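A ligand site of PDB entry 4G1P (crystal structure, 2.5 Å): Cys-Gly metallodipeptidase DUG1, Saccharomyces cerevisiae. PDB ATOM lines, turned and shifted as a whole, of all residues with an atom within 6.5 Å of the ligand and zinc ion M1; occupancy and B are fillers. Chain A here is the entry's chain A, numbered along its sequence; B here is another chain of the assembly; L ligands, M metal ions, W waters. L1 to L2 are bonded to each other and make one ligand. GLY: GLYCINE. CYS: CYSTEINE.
The guanidinium group (NH1) of Arg 348 is in hydrogen-bond range of an oxygen (O) of CYS L2. NE2 of His 233 of chain B sits close to N of GLY L1 (2.9 Å). SG of CYS L2 sits close to NE2 of His 385. SG of CYS L2 lies close to SG of Cys 218, 3.7 Å away.
A ring nitrogen (ND1) of His 450 lies within hydrogen-bond range of the side-chain hydroxyl of Thr 335 of chain B, 3.3 Å away. OE1 of Glu 172 sits at hydrogen-bond distance from NE2 of Gln 106, at 2.6 Å. The side-chain hydroxyl (OG) of Ser 422 is in hydrogen-bond range of the guanidinium group (NH1) of Arg 348 (2.7 Å). The side-chain hydroxyl (OG) of Ser 234 of chain B is in hydrogen-bond range of the guanidinium group (NH2) of Arg 348. N of Gly 235 of chain B sits at hydrogen-bond distance from ND1 of His 233 of chain B, at 2.8 Å. The backbone NH of Tyr 220 sits at hydrogen-bond distance from the backbone carbonyl oxygen of His 385 (2.8 Å). The side-chain carboxylate (OE1) of Glu 171 sits at hydrogen-bond distance from a ring nitrogen (NE2) of His 102. The backbone NH (N) of Ser 234 of chain B is in hydrogen-bond range of the backbone carbonyl oxygen (O) of Thr 335 of chain B, 3.3 Å away.
OE2 of Glu 171 sits close to O of GLY L1, at 3.1 Å. The backbone carbonyl oxygen (O) of Ser 422 sits close to an oxygen (O) of GLY L1, at 3.0 Å. Residues that only touch the ligand: Thr 335 of chain B. Hydrophobic or aromatic side chains within 4 Å of the ligand: His 385, His 450 and His 233 of chain B. Ten residues have an atom within 4 Å of the ligand: Asp 137, Glu 171, Glu 172, Cys 218, Arg 348, His 385, Ser 422, His 450, His 233 of chain B and Thr 335 of chain B. Along chain A the residues within 4 Å of the ligand span positions 137 to 450. The nearest printed residue that does not touch the ligand is Pro 424 (4.4 Å).
Three residues have an atom within 4 Å of zinc ion M1: Asp 137, Glu 172 and His 450. The nearest printed residue that does not touch zinc ion M1 is Glu 171 (4.02 Å).
Zinc ion M1 is bound by the side-chain carboxylate (OD2) of Asp 137, a ring nitrogen (NE2) of His 450, the side-chain carboxylate (OE2) of Glu 172 and a nitrogen (N) of GLY L1. Slightly farther from zinc ion M1 lies OE1 of Glu 172 (2.6 Å).
Water W2 bridges a sulfur (SG) of CYS L2 (3.0 Å) and the backbone carbonyl oxygen (O) of Cys 218 (3.4 Å).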
ATOM      1  N   HIS A 102      29.355 -19.016   8.704  1.00  0.00           N
ATOM      2  CA  HIS A 102      28.340 -19.580   9.582  1.00  0.00           C
ATOM      3  C   HIS A 102      28.483 -21.056   9.775  1.00  0.00           C
ATOM      4  O   HIS A 102      28.771 -21.807   8.825  1.00  0.00           O
ATOM      5  CB  HIS A 102      26.924 -19.206   9.121  1.00  0.00           C
ATOM      6  CG  HIS A 102      26.499 -19.849   7.834  1.00  0.00           C
ATOM      7  ND1 HIS A 102      25.883 -21.080   7.795  1.00  0.00           N
ATOM      8  CD2 HIS A 102      26.535 -19.409   6.554  1.00  0.00           C
ATOM      9  CE1 HIS A 102      25.592 -21.378   6.541  1.00  0.00           C
ATOM     10  NE2 HIS A 102      25.974 -20.381   5.767  1.00  0.00           N
ATOM     11  N   GLN A 106      21.712 -26.478   6.901  1.00  0.00           N
ATOM     12  CA  GLN A 106      20.382 -26.965   6.508  1.00  0.00           C
ATOM     13  C   GLN A 106      20.115 -28.383   7.038  1.00  0.00           C
ATOM     14  O   GLN A 106      21.035 -29.155   7.229  1.00  0.00           O
ATOM     15  CB  GLN A 106      20.263 -26.952   4.981  1.00  0.00           C
ATOM     16  CG  GLN A 106      20.134 -25.566   4.385  1.00  0.00           C
ATOM     17  CD  GLN A 106      18.769 -24.967   4.618  1.00  0.00           C
ATOM     18  OE1 GLN A 106      17.755 -25.604   4.351  1.00  0.00           O
ATOM     19  NE2 GLN A 106      18.729 -23.730   5.142  1.00  0.00           N
ATOM     20  N   ASP A 137      28.412 -25.124   2.476  1.00  0.00           N
ATOM     21  CA  ASP A 137      27.545 -24.084   2.996  1.00  0.00           C
ATOM     22  C   ASP A 137      27.290 -24.385   4.467  1.00  0.00           C
ATOM     23  O   ASP A 137      26.271 -25.004   4.783  1.00  0.00           O
ATOM     24  CB  ASP A 137      26.230 -24.085   2.192  1.00  0.00           C
ATOM     25  CG  ASP A 137      25.234 -23.043   2.672  1.00  0.00           C
ATOM     26  OD1 ASP A 137      25.604 -22.148   3.457  1.00  0.00           O
ATOM     27  OD2 ASP A 137      24.063 -23.093   2.239  1.00  0.00           O
ATOM     28  N   ASP A 138      28.176 -23.947   5.358  1.00  0.00           N
ATOM     29  CA  ASP A 138      29.286 -23.045   5.084  1.00  0.00           C
ATOM     30  C   ASP A 138      30.517 -23.487   5.876  1.00  0.00           C
ATOM     31  O   ASP A 138      31.427 -22.706   6.108  1.00  0.00           O
ATOM     32  CB  ASP A 138      28.888 -21.616   5.511  1.00  0.00           C
ATOM     33  CG  ASP A 138      29.920 -20.540   5.129  1.00  0.00           C
ATOM     34  OD1 ASP A 138      30.461 -20.563   4.000  1.00  0.00           O
ATOM     35  OD2 ASP A 138      30.190 -19.655   5.972  1.00  0.00           O
ATOM     36  N   GLU A 171      22.508 -18.615  10.469  1.00  0.00           N
ATOM     37  CA  GLU A 171      22.423 -18.121   9.101  1.00  0.00           C
ATOM     38  C   GLU A 171      21.310 -18.800   8.313  1.00  0.00           C
ATOM     39  O   GLU A 171      20.625 -18.162   7.520  1.00  0.00           O
ATOM     40  CB  GLU A 171      23.746 -18.252   8.359  1.00  0.00           C
ATOM     41  CG  GLU A 171      23.928 -17.301   7.183  1.00  0.00           C
ATOM     42  CD  GLU A 171      23.524 -17.899   5.840  1.00  0.00           C
ATOM     43  OE1 GLU A 171      23.003 -19.032   5.798  1.00  0.00           O
ATOM     44  OE2 GLU A 171      23.726 -17.213   4.803  1.00  0.00           O
ATOM     45  N   GLU A 172      21.109 -20.091   8.558  1.00  0.00           N
ATOM     46  CA  GLU A 172      20.078 -20.841   7.845  1.00  0.00           C
ATOM     47  C   GLU A 172      18.701 -20.617   8.484  1.00  0.00           C
ATOM     48  O   GLU A 172      17.713 -21.232   8.073  1.00  0.00           O
ATOM     49  CB  GLU A 172      20.427 -22.332   7.797  1.00  0.00           C
ATOM     50  CG  GLU A 172      21.798 -22.666   7.216  1.00  0.00           C
ATOM     51  CD  GLU A 172      21.856 -22.507   5.701  1.00  0.00           C
ATOM     52  OE1 GLU A 172      20.830 -22.147   5.089  1.00  0.00           O
ATOM     53  OE2 GLU A 172      22.936 -22.748   5.116  1.00  0.00           O
ATOM     54  N   SER A 173      18.651 -19.736   9.471  1.00  0.00           N
ATOM     55  CA  SER A 173      17.423 -19.467  10.218  1.00  0.00           C
ATOM     56  C   SER A 173      17.235 -17.959  10.457  1.00  0.00           C
ATOM     57  O   SER A 173      16.873 -17.532  11.556  1.00  0.00           O
ATOM     58  CB  SER A 173      17.444 -20.225  11.548  1.00  0.00           C
ATOM     59  OG  SER A 173      17.665 -21.611  11.353  1.00  0.00           O
ATOM     60  N   GLY A 174      17.518 -17.169   9.426  1.00  0.00           N
ATOM     61  CA  GLY A 174      17.286 -15.735   9.480  1.00  0.00           C
ATOM     62  C   GLY A 174      18.373 -14.861  10.078  1.00  0.00           C
ATOM     63  O   GLY A 174      18.192 -13.644  10.159  1.00  0.00           O
ATOM     64  N   ASP A 200      31.059 -17.390   1.388  1.00  0.00           N
ATOM     65  CA  ASP A 200      29.767 -18.002   1.666  1.00  0.00           C
ATOM     66  C   ASP A 200      28.907 -18.053   0.417  1.00  0.00           C
ATOM     67  O   ASP A 200      27.684 -17.894   0.485  1.00  0.00           O
ATOM     68  CB  ASP A 200      29.049 -17.197   2.744  1.00  0.00           C
ATOM     69  CG  ASP A 200      28.110 -18.043   3.585  1.00  0.00           C
ATOM     70  OD1 ASP A 200      27.962 -19.253   3.309  1.00  0.00           O
ATOM     71  OD2 ASP A 200      27.507 -17.503   4.526  1.00  0.00           O
ATOM     72  N   TYR A 202      29.427 -19.305  -4.172  1.00  0.00           N
ATOM     73  CA  TYR A 202      30.010 -20.286  -5.095  1.00  0.00           C
ATOM     74  C   TYR A 202      30.373 -19.628  -6.400  1.00  0.00           C
ATOM     75  O   TYR A 202      29.870 -18.547  -6.710  1.00  0.00           O
ATOM     76  CB  TYR A 202      29.010 -21.411  -5.371  1.00  0.00           C
ATOM     77  CG  TYR A 202      28.139 -21.642  -4.164  1.00  0.00           C
ATOM     78  CD1 TYR A 202      26.955 -20.931  -3.992  1.00  0.00           C
ATOM     79  CD2 TYR A 202      28.545 -22.507  -3.154  1.00  0.00           C
ATOM     80  CE1 TYR A 202      26.183 -21.093  -2.851  1.00  0.00           C
ATOM     81  CE2 TYR A 202      27.778 -22.683  -2.029  1.00  0.00           C
ATOM     82  CZ  TYR A 202      26.598 -21.987  -1.874  1.00  0.00           C
ATOM     83  OH  TYR A 202      25.831 -22.157  -0.731  1.00  0.00           O
ATOM     84  N   CYS A 218      16.395 -11.355   0.363  1.00  0.00           N
ATOM     85  CA  CYS A 218      15.393 -12.404   0.451  1.00  0.00           C
ATOM     86  C   CYS A 218      14.306 -12.055   1.474  1.00  0.00           C
ATOM     87  O   CYS A 218      14.588 -11.753   2.643  1.00  0.00           O
ATOM     88  CB  CYS A 218      16.044 -13.755   0.772  1.00  0.00           C
ATOM     89  SG  CYS A 218      14.889 -15.166   0.697  1.00  0.00           S
ATOM     90  N   ASN A 219      13.064 -12.072   1.021  1.00  0.00           N
ATOM     91  CA  ASN A 219      11.927 -11.882   1.918  1.00  0.00           C
ATOM     92  C   ASN A 219      11.118 -13.175   1.966  1.00  0.00           C
ATOM     93  O   ASN A 219      10.624 -13.650   0.932  1.00  0.00           O
ATOM     94  CB  ASN A 219      11.063 -10.695   1.476  1.00  0.00           C
ATOM     95  CG  ASN A 219      11.661  -9.361   1.882  1.00  0.00           C
ATOM     96  OD1 ASN A 219      12.871  -9.233   2.047  1.00  0.00           O
ATOM     97  ND2 ASN A 219      10.811  -8.360   2.046  1.00  0.00           N
ATOM     98  N   TYR A 220      11.018 -13.765   3.138  1.00  0.00           N
ATOM     99  CA  TYR A 220      10.360 -15.056   3.235  1.00  0.00           C
ATOM    100  C   TYR A 220       8.994 -14.904   3.897  1.00  0.00           C
ATOM    101  O   TYR A 220       8.897 -14.393   5.026  1.00  0.00           O
ATOM    102  CB  TYR A 220      11.227 -16.048   4.014  1.00  0.00           C
ATOM    103  CG  TYR A 220      10.940 -17.499   3.692  1.00  0.00           C
ATOM    104  CD1 TYR A 220       9.802 -18.120   4.170  1.00  0.00           C
ATOM    105  CD2 TYR A 220      11.810 -18.237   2.905  1.00  0.00           C
ATOM    106  CE1 TYR A 220       9.528 -19.444   3.870  1.00  0.00           C
ATOM    107  CE2 TYR A 220      11.558 -19.556   2.614  1.00  0.00           C
ATOM    108  CZ  TYR A 220      10.410 -20.158   3.096  1.00  0.00           C
ATOM    109  OH  TYR A 220      10.141 -21.480   2.827  1.00  0.00           O
ATOM    110  N   ARG A 348      13.224 -13.017  -3.965  1.00  0.00           N
ATOM    111  CA  ARG A 348      14.591 -12.537  -4.033  1.00  0.00           C
ATOM    112  C   ARG A 348      14.587 -11.072  -4.436  1.00  0.00           C
ATOM    113  O   ARG A 348      14.119 -10.725  -5.508  1.00  0.00           O
ATOM    114  CB  ARG A 348      15.406 -13.374  -5.019  1.00  0.00           C
ATOM    115  CG  ARG A 348      15.578 -14.836  -4.599  1.00  0.00           C
ATOM    116  CD  ARG A 348      16.502 -14.992  -3.399  1.00  0.00           C
ATOM    117  NE  ARG A 348      16.445 -16.351  -2.882  1.00  0.00           N
ATOM    118  CZ  ARG A 348      17.229 -16.832  -1.911  1.00  0.00           C
ATOM    119  NH1 ARG A 348      18.180 -16.083  -1.353  1.00  0.00           N
ATOM    120  NH2 ARG A 348      17.068 -18.099  -1.516  1.00  0.00           N
ATOM    121  N   HIS A 385      11.170 -13.876   7.610  1.00  0.00           N
ATOM    122  CA  HIS A 385      12.436 -13.155   7.739  1.00  0.00           C
ATOM    123  C   HIS A 385      12.756 -12.346   6.491  1.00  0.00           C
ATOM    124  O   HIS A 385      12.281 -12.654   5.392  1.00  0.00           O
ATOM    125  CB  HIS A 385      13.585 -14.086   8.124  1.00  0.00           C
ATOM    126  CG  HIS A 385      14.029 -15.010   7.038  1.00  0.00           C
ATOM    127  ND1 HIS A 385      14.032 -16.382   7.190  1.00  0.00           N
ATOM    128  CD2 HIS A 385      14.525 -14.777   5.795  1.00  0.00           C
ATOM    129  CE1 HIS A 385      14.486 -16.950   6.082  1.00  0.00           C
ATOM    130  NE2 HIS A 385      14.790 -15.995   5.218  1.00  0.00           N
ATOM    131  N   GLY A 420      22.767 -14.925  -7.113  1.00  0.00           N
ATOM    132  CA  GLY A 420      21.337 -15.144  -6.950  1.00  0.00           C
ATOM    133  C   GLY A 420      20.996 -15.381  -5.488  1.00  0.00           C
ATOM    134  O   GLY A 420      19.910 -15.032  -5.022  1.00  0.00           O
ATOM    135  N   GLY A 421      21.935 -15.971  -4.758  1.00  0.00           N
ATOM    136  CA  GLY A 421      21.739 -16.252  -3.348  1.00  0.00           C
ATOM    137  C   GLY A 421      21.858 -15.005  -2.494  1.00  0.00           C
ATOM    138  O   GLY A 421      22.017 -13.908  -3.033  1.00  0.00           O
ATOM    139  N   SER A 422      21.820 -15.189  -1.181  1.00  0.00           N
ATOM    140  CA  SER A 422      21.793 -14.084  -0.236  1.00  0.00           C
ATOM    141  C   SER A 422      22.688 -14.312   0.956  1.00  0.00           C
ATOM    142  O   SER A 422      22.824 -15.430   1.443  1.00  0.00           O
ATOM    143  CB  SER A 422      20.381 -13.889   0.265  1.00  0.00           C
ATOM    144  OG  SER A 422      19.509 -13.761  -0.821  1.00  0.00           O
ATOM    145  N   ILE A 423      23.308 -13.251   1.429  1.00  0.00           N
ATOM    146  CA  ILE A 423      24.006 -13.301   2.693  1.00  0.00           C
ATOM    147  C   ILE A 423      23.588 -12.072   3.469  1.00  0.00           C
ATOM    148  O   ILE A 423      24.257 -11.070   3.456  1.00  0.00           O
ATOM    149  CB  ILE A 423      25.517 -13.302   2.526  1.00  0.00           C
ATOM    150  CG1 ILE A 423      25.943 -14.411   1.564  1.00  0.00           C
ATOM    151  CG2 ILE A 423      26.179 -13.462   3.869  1.00  0.00           C
ATOM    152  CD1 ILE A 423      27.390 -14.314   1.093  1.00  0.00           C
ATOM    153  N   PRO A 424      22.437 -12.163   4.132  1.00  0.00           N
ATOM    154  CA  PRO A 424      21.775 -11.062   4.850  1.00  0.00           C
ATOM    155  C   PRO A 424      22.664  -9.989   5.513  1.00  0.00           C
ATOM    156  O   PRO A 424      22.356  -8.833   5.270  1.00  0.00           O
ATOM    157  CB  PRO A 424      20.936 -11.810   5.878  1.00  0.00           C
ATOM    158  CG  PRO A 424      20.505 -13.031   5.127  1.00  0.00           C
ATOM    159  CD  PRO A 424      21.663 -13.414   4.240  1.00  0.00           C
ATOM    160  N   ALA A 449      24.248 -27.030  -2.489  1.00  0.00           N
ATOM    161  CA  ALA A 449      23.819 -26.415  -1.240  1.00  0.00           C
ATOM    162  C   ALA A 449      22.285 -26.434  -1.129  1.00  0.00           C
ATOM    163  O   ALA A 449      21.581 -26.217  -2.122  1.00  0.00           O
ATOM    164  CB  ALA A 449      24.342 -24.997  -1.123  1.00  0.00           C
ATOM    165  N   HIS A 450      21.798 -26.736   0.073  1.00  0.00           N
ATOM    166  CA  HIS A 450      20.363 -26.818   0.371  1.00  0.00           C
ATOM    167  C   HIS A 450      19.701 -27.992  -0.338  1.00  0.00           C
ATOM    168  O   HIS A 450      18.477 -28.043  -0.465  1.00  0.00           O
ATOM    169  CB  HIS A 450      19.637 -25.514   0.014  1.00  0.00           C
ATOM    170  CG  HIS A 450      20.084 -24.339   0.821  1.00  0.00           C
ATOM    171  ND1 HIS A 450      19.307 -23.210   0.964  1.00  0.00           N
ATOM    172  CD2 HIS A 450      21.217 -24.107   1.522  1.00  0.00           C
ATOM    173  CE1 HIS A 450      19.943 -22.332   1.728  1.00  0.00           C
ATOM    174  NE2 HIS A 450      21.105 -22.858   2.075  1.00  0.00           N
ATOM    175  N   HIS B 233      18.641 -24.877  -4.644  1.00  0.00           N
ATOM    176  CA  HIS B 233      18.719 -23.686  -3.802  1.00  0.00           C
ATOM    177  C   HIS B 233      17.863 -22.617  -4.480  1.00  0.00           C
ATOM    178  O   HIS B 233      18.077 -22.296  -5.640  1.00  0.00           O
ATOM    179  CB  HIS B 233      20.173 -23.232  -3.695  1.00  0.00           C
ATOM    180  CG  HIS B 233      20.390 -22.081  -2.760  1.00  0.00           C
ATOM    181  ND1 HIS B 233      19.880 -20.825  -3.011  1.00  0.00           N
ATOM    182  CD2 HIS B 233      21.042 -22.002  -1.578  1.00  0.00           C
ATOM    183  CE1 HIS B 233      20.227 -20.016  -2.019  1.00  0.00           C
ATOM    184  NE2 HIS B 233      20.925 -20.704  -1.136  1.00  0.00           N
ATOM    185  N   SER B 234      16.878 -22.090  -3.769  1.00  0.00           N
ATOM    186  CA  SER B 234      15.914 -21.243  -4.456  1.00  0.00           C
ATOM    187  C   SER B 234      16.481 -19.876  -4.828  1.00  0.00           C
ATOM    188  O   SER B 234      15.830 -19.132  -5.552  1.00  0.00           O
ATOM    189  CB  SER B 234      14.600 -21.092  -3.669  1.00  0.00           C
ATOM    190  OG  SER B 234      14.747 -20.162  -2.618  1.00  0.00           O
ATOM    191  N   GLY B 235      17.689 -19.583  -4.328  1.00  0.00           N
ATOM    192  CA  GLY B 235      18.350 -18.318  -4.595  1.00  0.00           C
ATOM    193  C   GLY B 235      19.271 -18.410  -5.793  1.00  0.00           C
ATOM    194  O   GLY B 235      19.287 -17.544  -6.654  1.00  0.00           O
ATOM    195  N   THR B 335      14.516 -22.271   1.954  1.00  0.00           N
ATOM    196  CA  THR B 335      14.688 -21.653   0.645  1.00  0.00           C
ATOM    197  C   THR B 335      15.101 -22.724  -0.329  1.00  0.00           C
ATOM    198  O   THR B 335      16.290 -22.871  -0.642  1.00  0.00           O
ATOM    199  CB  THR B 335      15.762 -20.584   0.665  1.00  0.00           C
ATOM    200  OG1 THR B 335      16.849 -21.015   1.478  1.00  0.00           O
ATOM    201  CG2 THR B 335      15.225 -19.292   1.223  1.00  0.00           C
HETATM  202  N   GLY L   1      22.380 -20.231   1.363  1.00  0.00           N
HETATM  203  CA  GLY L   1      22.342 -19.754   2.734  1.00  0.00           C
HETATM  204  C   GLY L   1      21.172 -18.811   2.787  1.00  0.00           C
HETATM  205  O   GLY L   1      21.336 -17.588   2.838  1.00  0.00           O
HETATM  206  N   CYS L   2      19.976 -19.394   2.759  1.00  0.00           N
HETATM  207  CA  CYS L   2      18.755 -18.656   2.501  1.00  0.00           C
HETATM  208  C   CYS L   2      18.760 -18.166   1.048  1.00  0.00           C
HETATM  209  O   CYS L   2      19.694 -17.508   0.605  1.00  0.00           O
HETATM  210  CB  CYS L   2      18.600 -17.495   3.494  1.00  0.00           C
HETATM  211  SG  CYS L   2      17.114 -16.566   3.296  1.00  0.00           S
HETATM  212 ZN    ZN M   1      22.605 -22.061   3.184  1.00  0.00          ZN
HETATM  213 ZN    ZN M   2      25.559 -19.646   2.066  1.00  0.00          ZN
HETATM  214  O   HOH W   1      17.947 -18.041   6.798  1.00  0.00           O
HETATM  215  O   HOH W   2      17.232 -13.588   3.723  1.00  0.00           O
